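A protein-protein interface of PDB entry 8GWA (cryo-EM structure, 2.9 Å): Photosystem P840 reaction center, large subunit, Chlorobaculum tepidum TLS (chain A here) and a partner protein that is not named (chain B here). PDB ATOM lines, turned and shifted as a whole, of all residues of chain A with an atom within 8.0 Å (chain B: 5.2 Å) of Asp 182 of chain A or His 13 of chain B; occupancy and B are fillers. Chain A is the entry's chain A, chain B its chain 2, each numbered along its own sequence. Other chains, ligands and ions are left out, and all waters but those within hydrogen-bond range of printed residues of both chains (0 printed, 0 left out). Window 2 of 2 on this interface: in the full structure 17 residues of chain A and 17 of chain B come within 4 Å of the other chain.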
ATOM      1  N   CYS A 177      16.967   5.934 -15.123  1.00  0.00           N
ATOM      2  CA  CYS A 177      16.076   5.829 -16.267  1.00  0.00           C
ATOM      3  C   CYS A 177      15.618   7.220 -16.674  1.00  0.00           C
ATOM      4  O   CYS A 177      15.270   8.048 -15.828  1.00  0.00           O
ATOM      5  CB  CYS A 177      14.859   4.944 -15.964  1.00  0.00           C
ATOM      6  SG  CYS A 177      13.744   4.713 -17.367  1.00  0.00           S
ATOM      7  N   GLY A 178      15.622   7.469 -17.979  1.00  0.00           N
ATOM      8  CA  GLY A 178      15.167   8.730 -18.526  1.00  0.00           C
ATOM      9  C   GLY A 178      13.660   8.742 -18.697  1.00  0.00           C
ATOM     10  O   GLY A 178      13.032   7.702 -18.873  1.00  0.00           O
ATOM     11  N   ASN A 179      13.085   9.938 -18.642  1.00  0.00           N
ATOM     12  CA  ASN A 179      11.646  10.124 -18.772  1.00  0.00           C
ATOM     13  C   ASN A 179      11.346  10.711 -20.144  1.00  0.00           C
ATOM     14  O   ASN A 179      11.781  11.823 -20.454  1.00  0.00           O
ATOM     15  CB  ASN A 179      11.114  11.035 -17.666  1.00  0.00           C
ATOM     16  CG  ASN A 179       9.600  11.044 -17.596  1.00  0.00           C
ATOM     17  OD1 ASN A 179       8.948  10.046 -17.897  1.00  0.00           O
ATOM     18  ND2 ASN A 179       9.034  12.177 -17.198  1.00  0.00           N
ATOM     19  N   PHE A 180      10.594   9.968 -20.958  1.00  0.00           N
ATOM     20  CA  PHE A 180      10.267  10.447 -22.296  1.00  0.00           C
ATOM     21  C   PHE A 180       9.412  11.705 -22.254  1.00  0.00           C
ATOM     22  O   PHE A 180       9.569  12.587 -23.107  1.00  0.00           O
ATOM     23  CB  PHE A 180       9.554   9.351 -23.090  1.00  0.00           C
ATOM     24  CG  PHE A 180       9.315   9.706 -24.528  1.00  0.00           C
ATOM     25  CD1 PHE A 180      10.341   9.641 -25.454  1.00  0.00           C
ATOM     26  CD2 PHE A 180       8.060  10.111 -24.955  1.00  0.00           C
ATOM     27  CE1 PHE A 180      10.121   9.970 -26.776  1.00  0.00           C
ATOM     28  CE2 PHE A 180       7.836  10.441 -26.276  1.00  0.00           C
ATOM     29  CZ  PHE A 180       8.867  10.370 -27.188  1.00  0.00           C
ATOM     30  N   ARG A 181       8.504  11.807 -21.284  1.00  0.00           N
ATOM     31  CA  ARG A 181       7.615  12.960 -21.222  1.00  0.00           C
ATOM     32  C   ARG A 181       8.333  14.208 -20.721  1.00  0.00           C
ATOM     33  O   ARG A 181       8.124  15.302 -21.257  1.00  0.00           O
ATOM     34  CB  ARG A 181       6.411  12.641 -20.338  1.00  0.00           C
ATOM     35  CG  ARG A 181       5.228  12.074 -21.102  1.00  0.00           C
ATOM     36  CD  ARG A 181       4.503  11.031 -20.277  1.00  0.00           C
ATOM     37  NE  ARG A 181       3.568  11.643 -19.342  1.00  0.00           N
ATOM     38  CZ  ARG A 181       2.876  10.975 -18.431  1.00  0.00           C
ATOM     39  NH1 ARG A 181       2.987   9.663 -18.306  1.00  0.00           N
ATOM     40  NH2 ARG A 181       2.054  11.639 -17.625  1.00  0.00           N
ATOM     41  N   ASP A 182       9.186  14.071 -19.705  1.00  0.00           N
ATOM     42  CA  ASP A 182       9.913  15.210 -19.142  1.00  0.00           C
ATOM     43  C   ASP A 182      11.380  14.819 -18.999  1.00  0.00           C
ATOM     44  O   ASP A 182      11.763  14.182 -18.013  1.00  0.00           O
ATOM     45  CB  ASP A 182       9.322  15.639 -17.804  1.00  0.00           C
ATOM     46  CG  ASP A 182       9.596  17.097 -17.489  1.00  0.00           C
ATOM     47  OD1 ASP A 182       9.734  17.897 -18.438  1.00  0.00           O
ATOM     48  OD2 ASP A 182       9.672  17.445 -16.291  1.00  0.00           O
ATOM     49  N   PHE A 183      12.198  15.205 -19.977  1.00  0.00           N
ATOM     50  CA  PHE A 183      13.624  14.919 -19.946  1.00  0.00           C
ATOM     51  C   PHE A 183      14.421  16.182 -20.226  1.00  0.00           C
ATOM     52  O   PHE A 183      14.045  16.994 -21.077  1.00  0.00           O
ATOM     53  CB  PHE A 183      14.017  13.841 -20.970  1.00  0.00           C
ATOM     54  CG  PHE A 183      13.703  14.205 -22.397  1.00  0.00           C
ATOM     55  CD1 PHE A 183      12.479  13.884 -22.958  1.00  0.00           C
ATOM     56  CD2 PHE A 183      14.647  14.842 -23.187  1.00  0.00           C
ATOM     57  CE1 PHE A 183      12.196  14.215 -24.269  1.00  0.00           C
ATOM     58  CE2 PHE A 183      14.369  15.173 -24.497  1.00  0.00           C
ATOM     59  CZ  PHE A 183      13.143  14.858 -25.038  1.00  0.00           C
ATOM     60  N   ARG A 184      15.515  16.348 -19.492  1.00  0.00           N
ATOM     61  CA  ARG A 184      16.587  17.218 -19.949  1.00  0.00           C
ATOM     62  C   ARG A 184      17.157  16.678 -21.256  1.00  0.00           C
ATOM     63  O   ARG A 184      17.361  15.470 -21.414  1.00  0.00           O
ATOM     64  CB  ARG A 184      17.670  17.338 -18.869  1.00  0.00           C
ATOM     65  CG  ARG A 184      18.670  16.183 -18.796  1.00  0.00           C
ATOM     66  CD  ARG A 184      17.994  14.902 -18.306  1.00  0.00           C
ATOM     67  NE  ARG A 184      18.918  13.784 -18.152  1.00  0.00           N
ATOM     68  CZ  ARG A 184      19.290  12.980 -19.137  1.00  0.00           C
ATOM     69  NH1 ARG A 184      18.829  13.134 -20.367  1.00  0.00           N
ATOM     70  NH2 ARG A 184      20.141  11.991 -18.880  1.00  0.00           N
ATOM     71  N   PHE A 185      17.360  17.573 -22.224  1.00  0.00           N
ATOM     72  CA  PHE A 185      17.817  17.156 -23.544  1.00  0.00           C
ATOM     73  C   PHE A 185      19.203  16.524 -23.473  1.00  0.00           C
ATOM     74  O   PHE A 185      19.362  15.334 -23.766  1.00  0.00           O
ATOM     75  CB  PHE A 185      17.817  18.344 -24.512  1.00  0.00           C
ATOM     76  CG  PHE A 185      18.246  17.995 -25.916  1.00  0.00           C
ATOM     77  CD1 PHE A 185      18.129  16.701 -26.403  1.00  0.00           C
ATOM     78  CD2 PHE A 185      18.763  18.970 -26.753  1.00  0.00           C
ATOM     79  CE1 PHE A 185      18.530  16.388 -27.687  1.00  0.00           C
ATOM     80  CE2 PHE A 185      19.159  18.663 -28.041  1.00  0.00           C
ATOM     81  CZ  PHE A 185      19.042  17.371 -28.508  1.00  0.00           C
ATOM     82  N   ASN A 195      14.650  24.952 -21.024  1.00  0.00           N
ATOM     83  CA  ASN A 195      15.006  24.976 -19.606  1.00  0.00           C
ATOM     84  C   ASN A 195      14.220  23.903 -18.853  1.00  0.00           C
ATOM     85  O   ASN A 195      13.226  24.146 -18.164  1.00  0.00           O
ATOM     86  CB  ASN A 195      14.812  26.390 -19.052  1.00  0.00           C
ATOM     87  CG  ASN A 195      13.364  26.883 -19.115  1.00  0.00           C
ATOM     88  OD1 ASN A 195      12.442  26.148 -19.467  1.00  0.00           O
ATOM     89  ND2 ASN A 195      13.168  28.148 -18.766  1.00  0.00           N
ATOM     90  N   GLY A 196      14.736  22.679 -18.943  1.00  0.00           N
ATOM     91  CA  GLY A 196      13.953  21.520 -18.596  1.00  0.00           C
ATOM     92  C   GLY A 196      12.789  21.415 -19.559  1.00  0.00           C
ATOM     93  O   GLY A 196      12.872  21.822 -20.723  1.00  0.00           O
ATOM     94  N   THR A 197      11.681  20.869 -19.063  1.00  0.00           N
ATOM     95  CA  THR A 197      10.386  20.956 -19.734  1.00  0.00           C
ATOM     96  C   THR A 197      10.468  20.456 -21.178  1.00  0.00           C
ATOM     97  O   THR A 197      10.268  21.204 -22.131  1.00  0.00           O
ATOM     98  CB  THR A 197       9.855  22.393 -19.714  1.00  0.00           C
ATOM     99  OG1 THR A 197      10.516  23.157 -20.731  1.00  0.00           O
ATOM    100  CG2 THR A 197      10.114  23.036 -18.375  1.00  0.00           C
ATOM    101  N   SER A 198      10.790  19.174 -21.319  1.00  0.00           N
ATOM    102  CA  SER A 198      10.805  18.589 -22.651  1.00  0.00           C
ATOM    103  C   SER A 198       9.419  18.697 -23.273  1.00  0.00           C
ATOM    104  O   SER A 198       8.405  18.740 -22.572  1.00  0.00           O
ATOM    105  CB  SER A 198      11.242  17.130 -22.602  1.00  0.00           C
ATOM    106  OG  SER A 198      10.260  16.331 -21.977  1.00  0.00           O
ATOM    107  N   ALA A 199       9.383  18.762 -24.602  1.00  0.00           N
ATOM    108  CA  ALA A 199       8.132  19.020 -25.301  1.00  0.00           C
ATOM    109  C   ALA A 199       7.099  17.950 -24.977  1.00  0.00           C
ATOM    110  O   ALA A 199       7.382  16.750 -25.044  1.00  0.00           O
ATOM    111  CB  ALA A 199       8.377  19.080 -26.807  1.00  0.00           C
ATOM    112  N   LYS A 200       5.894  18.394 -24.623  1.00  0.00           N
ATOM    113  CA  LYS A 200       4.806  17.494 -24.279  1.00  0.00           C
ATOM    114  C   LYS A 200       3.860  17.242 -25.442  1.00  0.00           C
ATOM    115  O   LYS A 200       3.104  16.266 -25.408  1.00  0.00           O
ATOM    116  CB  LYS A 200       4.004  18.057 -23.099  1.00  0.00           C
ATOM    117  CG  LYS A 200       4.858  18.538 -21.939  1.00  0.00           C
ATOM    118  CD  LYS A 200       5.756  17.438 -21.411  1.00  0.00           C
ATOM    119  CE  LYS A 200       6.338  17.810 -20.058  1.00  0.00           C
ATOM    120  NZ  LYS A 200       7.824  17.750 -20.055  1.00  0.00           N
ATOM    121  N   GLU A 204       4.588  21.590 -29.836  1.00  0.00           N
ATOM    122  CA  GLU A 204       5.646  22.000 -28.928  1.00  0.00           C
ATOM    123  C   GLU A 204       6.958  21.286 -29.225  1.00  0.00           C
ATOM    124  O   GLU A 204       8.008  21.721 -28.742  1.00  0.00           O
ATOM    125  CB  GLU A 204       5.198  21.748 -27.482  1.00  0.00           C
ATOM    126  CG  GLU A 204       6.161  22.202 -26.400  1.00  0.00           C
ATOM    127  CD  GLU A 204       5.620  21.964 -25.004  1.00  0.00           C
ATOM    128  OE1 GLU A 204       4.502  21.424 -24.883  1.00  0.00           O
ATOM    129  OE2 GLU A 204       6.314  22.319 -24.027  1.00  0.00           O
ATOM    130  N   TRP A 261      10.022  27.199 -29.990  1.00  0.00           N
ATOM    131  CA  TRP A 261       9.979  26.686 -28.629  1.00  0.00           C
ATOM    132  C   TRP A 261       9.248  27.652 -27.712  1.00  0.00           C
ATOM    133  O   TRP A 261       8.410  27.239 -26.903  1.00  0.00           O
ATOM    134  CB  TRP A 261      11.395  26.436 -28.114  1.00  0.00           C
ATOM    135  CG  TRP A 261      11.428  25.940 -26.707  1.00  0.00           C
ATOM    136  CD1 TRP A 261      12.071  26.513 -25.652  1.00  0.00           C
ATOM    137  CD2 TRP A 261      10.791  24.764 -26.199  1.00  0.00           C
ATOM    138  NE1 TRP A 261      11.873  25.767 -24.516  1.00  0.00           N
ATOM    139  CE2 TRP A 261      11.090  24.688 -24.826  1.00  0.00           C
ATOM    140  CE3 TRP A 261       9.995  23.770 -26.770  1.00  0.00           C
ATOM    141  CZ2 TRP A 261      10.622  23.659 -24.020  1.00  0.00           C
ATOM    142  CZ3 TRP A 261       9.536  22.750 -25.971  1.00  0.00           C
ATOM    143  CH2 TRP A 261       9.846  22.700 -24.612  1.00  0.00           C
ATOM    144  N   THR B  11       5.451  22.746 -14.286  1.00  0.00           N
ATOM    145  CA  THR B  11       4.879  21.702 -15.124  1.00  0.00           C
ATOM    146  C   THR B  11       4.052  20.743 -14.277  1.00  0.00           C
ATOM    147  O   THR B  11       4.409  20.431 -13.137  1.00  0.00           O
ATOM    148  CB  THR B  11       5.976  20.948 -15.884  1.00  0.00           C
ATOM    149  OG1 THR B  11       5.377  20.044 -16.823  1.00  0.00           O
ATOM    150  CG2 THR B  11       6.885  20.179 -14.934  1.00  0.00           C
ATOM    151  N   ALA B  12       2.927  20.303 -14.832  1.00  0.00           N
ATOM    152  CA  ALA B  12       1.982  19.444 -14.133  1.00  0.00           C
ATOM    153  C   ALA B  12       2.047  18.042 -14.722  1.00  0.00           C
ATOM    154  O   ALA B  12       1.651  17.829 -15.872  1.00  0.00           O
ATOM    155  CB  ALA B  12       0.562  20.000 -14.229  1.00  0.00           C
ATOM    156  N   HIS B  13       2.543  17.094 -13.935  1.00  0.00           N
ATOM    157  CA  HIS B  13       2.595  15.693 -14.321  1.00  0.00           C
ATOM    158  C   HIS B  13       1.424  14.954 -13.692  1.00  0.00           C
ATOM    159  O   HIS B  13       1.097  15.178 -12.523  1.00  0.00           O
ATOM    160  CB  HIS B  13       3.912  15.047 -13.887  1.00  0.00           C
ATOM    161  CG  HIS B  13       5.127  15.775 -14.370  1.00  0.00           C
ATOM    162  ND1 HIS B  13       5.304  16.136 -15.687  1.00  0.00           N
ATOM    163  CD2 HIS B  13       6.227  16.210 -13.711  1.00  0.00           C
ATOM    164  CE1 HIS B  13       6.460  16.762 -15.819  1.00  0.00           C
ATOM    165  NE2 HIS B  13       7.039  16.819 -14.635  1.00  0.00           N
ATOM    166  N   SER B  14       0.789  14.081 -14.470  1.00  0.00           N
ATOM    167  CA  SER B  14      -0.356  13.332 -13.972  1.00  0.00           C
ATOM    168  C   SER B  14      -0.591  12.114 -14.852  1.00  0.00           C
ATOM    169  O   SER B  14      -0.547  12.215 -16.081  1.00  0.00           O
ATOM    170  CB  SER B  14      -1.611  14.209 -13.929  1.00  0.00           C
ATOM    171  OG  SER B  14      -1.815  14.869 -15.165  1.00  0.00           O
ATOM    172  N   ASP B  15      -0.840  10.970 -14.218  1.00  0.00           N
ATOM    173  CA  ASP B  15      -1.167   9.728 -14.903  1.00  0.00           C
ATOM    174  C   ASP B  15      -2.488   9.205 -14.365  1.00  0.00           C
ATOM    175  O   ASP B  15      -2.628   9.000 -13.156  1.00  0.00           O
ATOM    176  CB  ASP B  15      -0.072   8.677 -14.705  1.00  0.00           C
ATOM    177  CG  ASP B  15       1.093   8.866 -15.649  1.00  0.00           C
ATOM    178  OD1 ASP B  15       1.227   9.974 -16.206  1.00  0.00           O
ATOM    179  OD2 ASP B  15       1.872   7.908 -15.837  1.00  0.00           O
ATOM    180  N   ARG B  33      -2.087   9.367 -10.314  1.00  0.00           N
ATOM    181  CA  ARG B  33      -1.022  10.062  -9.612  1.00  0.00           C
ATOM    182  C   ARG B  33      -0.811  11.406 -10.290  1.00  0.00           C
ATOM    183  O   ARG B  33      -1.046  11.548 -11.492  1.00  0.00           O
ATOM    184  CB  ARG B  33       0.286   9.260  -9.623  1.00  0.00           C
ATOM    185  CG  ARG B  33       0.328   8.115  -8.625  1.00  0.00           C
ATOM    186  CD  ARG B  33      -0.214   6.840  -9.249  1.00  0.00           C
ATOM    187  NE  ARG B  33      -0.019   5.676  -8.394  1.00  0.00           N
ATOM    188  CZ  ARG B  33      -0.930   5.205  -7.553  1.00  0.00           C
ATOM    189  NH1 ARG B  33      -2.116   5.777  -7.425  1.00  0.00           N
ATOM    190  NH2 ARG B  33      -0.644   4.130  -6.824  1.00  0.00           N
ATOM    191  N   ALA B  34      -0.375  12.396  -9.518  1.00  0.00           N
ATOM    192  CA  ALA B  34      -0.200  13.730 -10.071  1.00  0.00           C
ATOM    193  C   ALA B  34       0.950  14.442  -9.377  1.00  0.00           C
ATOM    194  O   ALA B  34       1.121  14.327  -8.161  1.00  0.00           O
ATOM    195  CB  ALA B  34      -1.481  14.559  -9.945  1.00  0.00           C
ATOM    196  N   LYS B  35       1.732  15.176 -10.164  1.00  0.00           N
ATOM    197  CA  LYS B  35       2.812  16.014  -9.662  1.00  0.00           C
ATOM    198  C   LYS B  35       2.593  17.430 -10.168  1.00  0.00           C
ATOM    199  O   LYS B  35       2.446  17.642 -11.375  1.00  0.00           O
ATOM    200  CB  LYS B  35       4.181  15.502 -10.122  1.00  0.00           C
ATOM    201  CG  LYS B  35       4.515  14.094  -9.667  1.00  0.00           C
ATOM    202  CD  LYS B  35       4.660  14.013  -8.161  1.00  0.00           C
ATOM    203  CE  LYS B  35       5.159  12.642  -7.741  1.00  0.00           C
ATOM    204  NZ  LYS B  35       4.131  11.588  -7.971  1.00  0.00           N
ATOM    205  N   VAL B  36       2.570  18.392  -9.252  1.00  0.00           N
ATOM    206  CA  VAL B  36       2.400  19.801  -9.593  1.00  0.00           C
ATOM    207  C   VAL B  36       3.546  20.575  -8.964  1.00  0.00           C
ATOM    208  O   VAL B  36       3.783  20.466  -7.756  1.00  0.00           O
ATOM    209  CB  VAL B  36       1.049  20.356  -9.113  1.00  0.00           C
ATOM    210  CG1 VAL B  36       0.827  21.748  -9.673  1.00  0.00           C
ATOM    211  CG2 VAL B  36      -0.085  19.430  -9.520  1.00  0.00           C
ATOM    212  N   ASP B 310       1.421  17.505 -18.821  1.00  0.00           N
ATOM    213  CA  ASP B 310       1.561  16.270 -19.589  1.00  0.00           C
ATOM    214  C   ASP B 310       0.742  15.175 -18.904  1.00  0.00           C
ATOM    215  O   ASP B 310       1.258  14.327 -18.173  1.00  0.00           O
ATOM    216  CB  ASP B 310       3.083  15.890 -19.786  1.00  0.00           C
ATOM    217  CG  ASP B 310       3.820  15.625 -18.479  1.00  0.00           C
ATOM    218  OD1 ASP B 310       3.222  15.764 -17.396  1.00  0.00           O
ATOM    219  OD2 ASP B 310       5.015  15.268 -18.542  1.00  0.00           O
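NE2 of His 13 of chain B lies within hydrogen-bond range of OD2 of Asp 182 of chain A.
The side-chain carboxylate (OD2) of Asp 310 of chain B is in salt-bridge range of the guanidinium group (NE) of Arg 181 of chain A (3.98 Å).
The backbone carbonyl oxygen (O) of Ser 14 of chain B is in hydrogen-bond range of the guanidinium group (NH2) of Arg 181 of chain A (3.1 Å).
The guanidinium group (NH1) of Arg 181 of chain A is in salt-bridge range of the side-chain carboxylate (OD1) of Asp 15 of chain B, at 2.8 Å.
Cys 177 of chain A touches none of the printed residues of chain B.
Of the printed residues of chain B, Arg 181 of chain A touches Ser 14 (3.1 Å), Asp 15 (2.3 Å) and Asp 310 (2.9 Å).
Asp 182 of chain A touches just one residue of chain B: His 13 (3.2 Å).
Of the printed residues of chain B, Lys 200 of chain A touches Asp 310.
No residue of chain A comes within 4 Å of Ala 12 of chain B.
His 13 of chain B touches just one residue of chain A: Asp 182.
Of the printed residues of chain A, Ser 14 of chain B touches Arg 181.
Of the printed residues of chain A, Asp 15 of chain B touches Arg 181.
Arg 33 of chain B touches none of the printed residues of chain A.
Printed residues of chain A within 4 Å of Asp 310 of chain B: Arg 181 (2.9 Å) and Lys 200 (3.2 Å).
The nearest residue of chain A that does not touch His 13 of chain B is Lys 200 of chain A (4.4 Å).
The nearest printed residue of chain A that does not touch Ser 14 of chain B is Lys 200 of chain A (8.7 Å).
Of the 17 printed residues of chain A, 3 touch a printed residue of chain B.
Printed residues of chain B that touch a printed residue of chain A: His 13, Ser 14, Asp 15 and Asp 310.
Along chain B the printed residues that touch a printed residue of chain A span positions 13 to 310.
Among the printed residues, 5 pairs touch across the chains.
Among the printed residues, Asp or Glu carboxylates within 4 Å of a Lys or Arg side-chain nitrogen of the other chain: Arg 181 of chain A with Asp 15 of chain B and Arg 181 of chain A with Asp 310 of chain B.
O of Ala 12 of chain B lies within hydrogen-bond range of N of Asp 310 of chain B (3.0 Å).
A ring nitrogen (ND1) of His 13 of chain B lies within hydrogen-bond range of the side-chain carboxylate of Asp 310 of chain B (2.7 Å).
The backbone carbonyl oxygen of Arg 181 of chain A sits at hydrogen-bond distance from the side-chain amino group of Lys 200 of chain A (2.7 Å).
The side-chain carboxylate (OD1) of Asp 182 of chain A sits at hydrogen-bond distance from the backbone NH (N) of Ser 198 of chain A, at 3.3 Å.
N of Asp 15 of chain B lies within hydrogen-bond range of O of Arg 33 of chain B.
NZ of Lys 200 of chain A sits at hydrogen-bond distance from O of Ser 198 of chain A.
Among the printed residues, merely in contact across the chains: Lys 200 of chain A with Asp 310 of chain B (3.2 Å).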
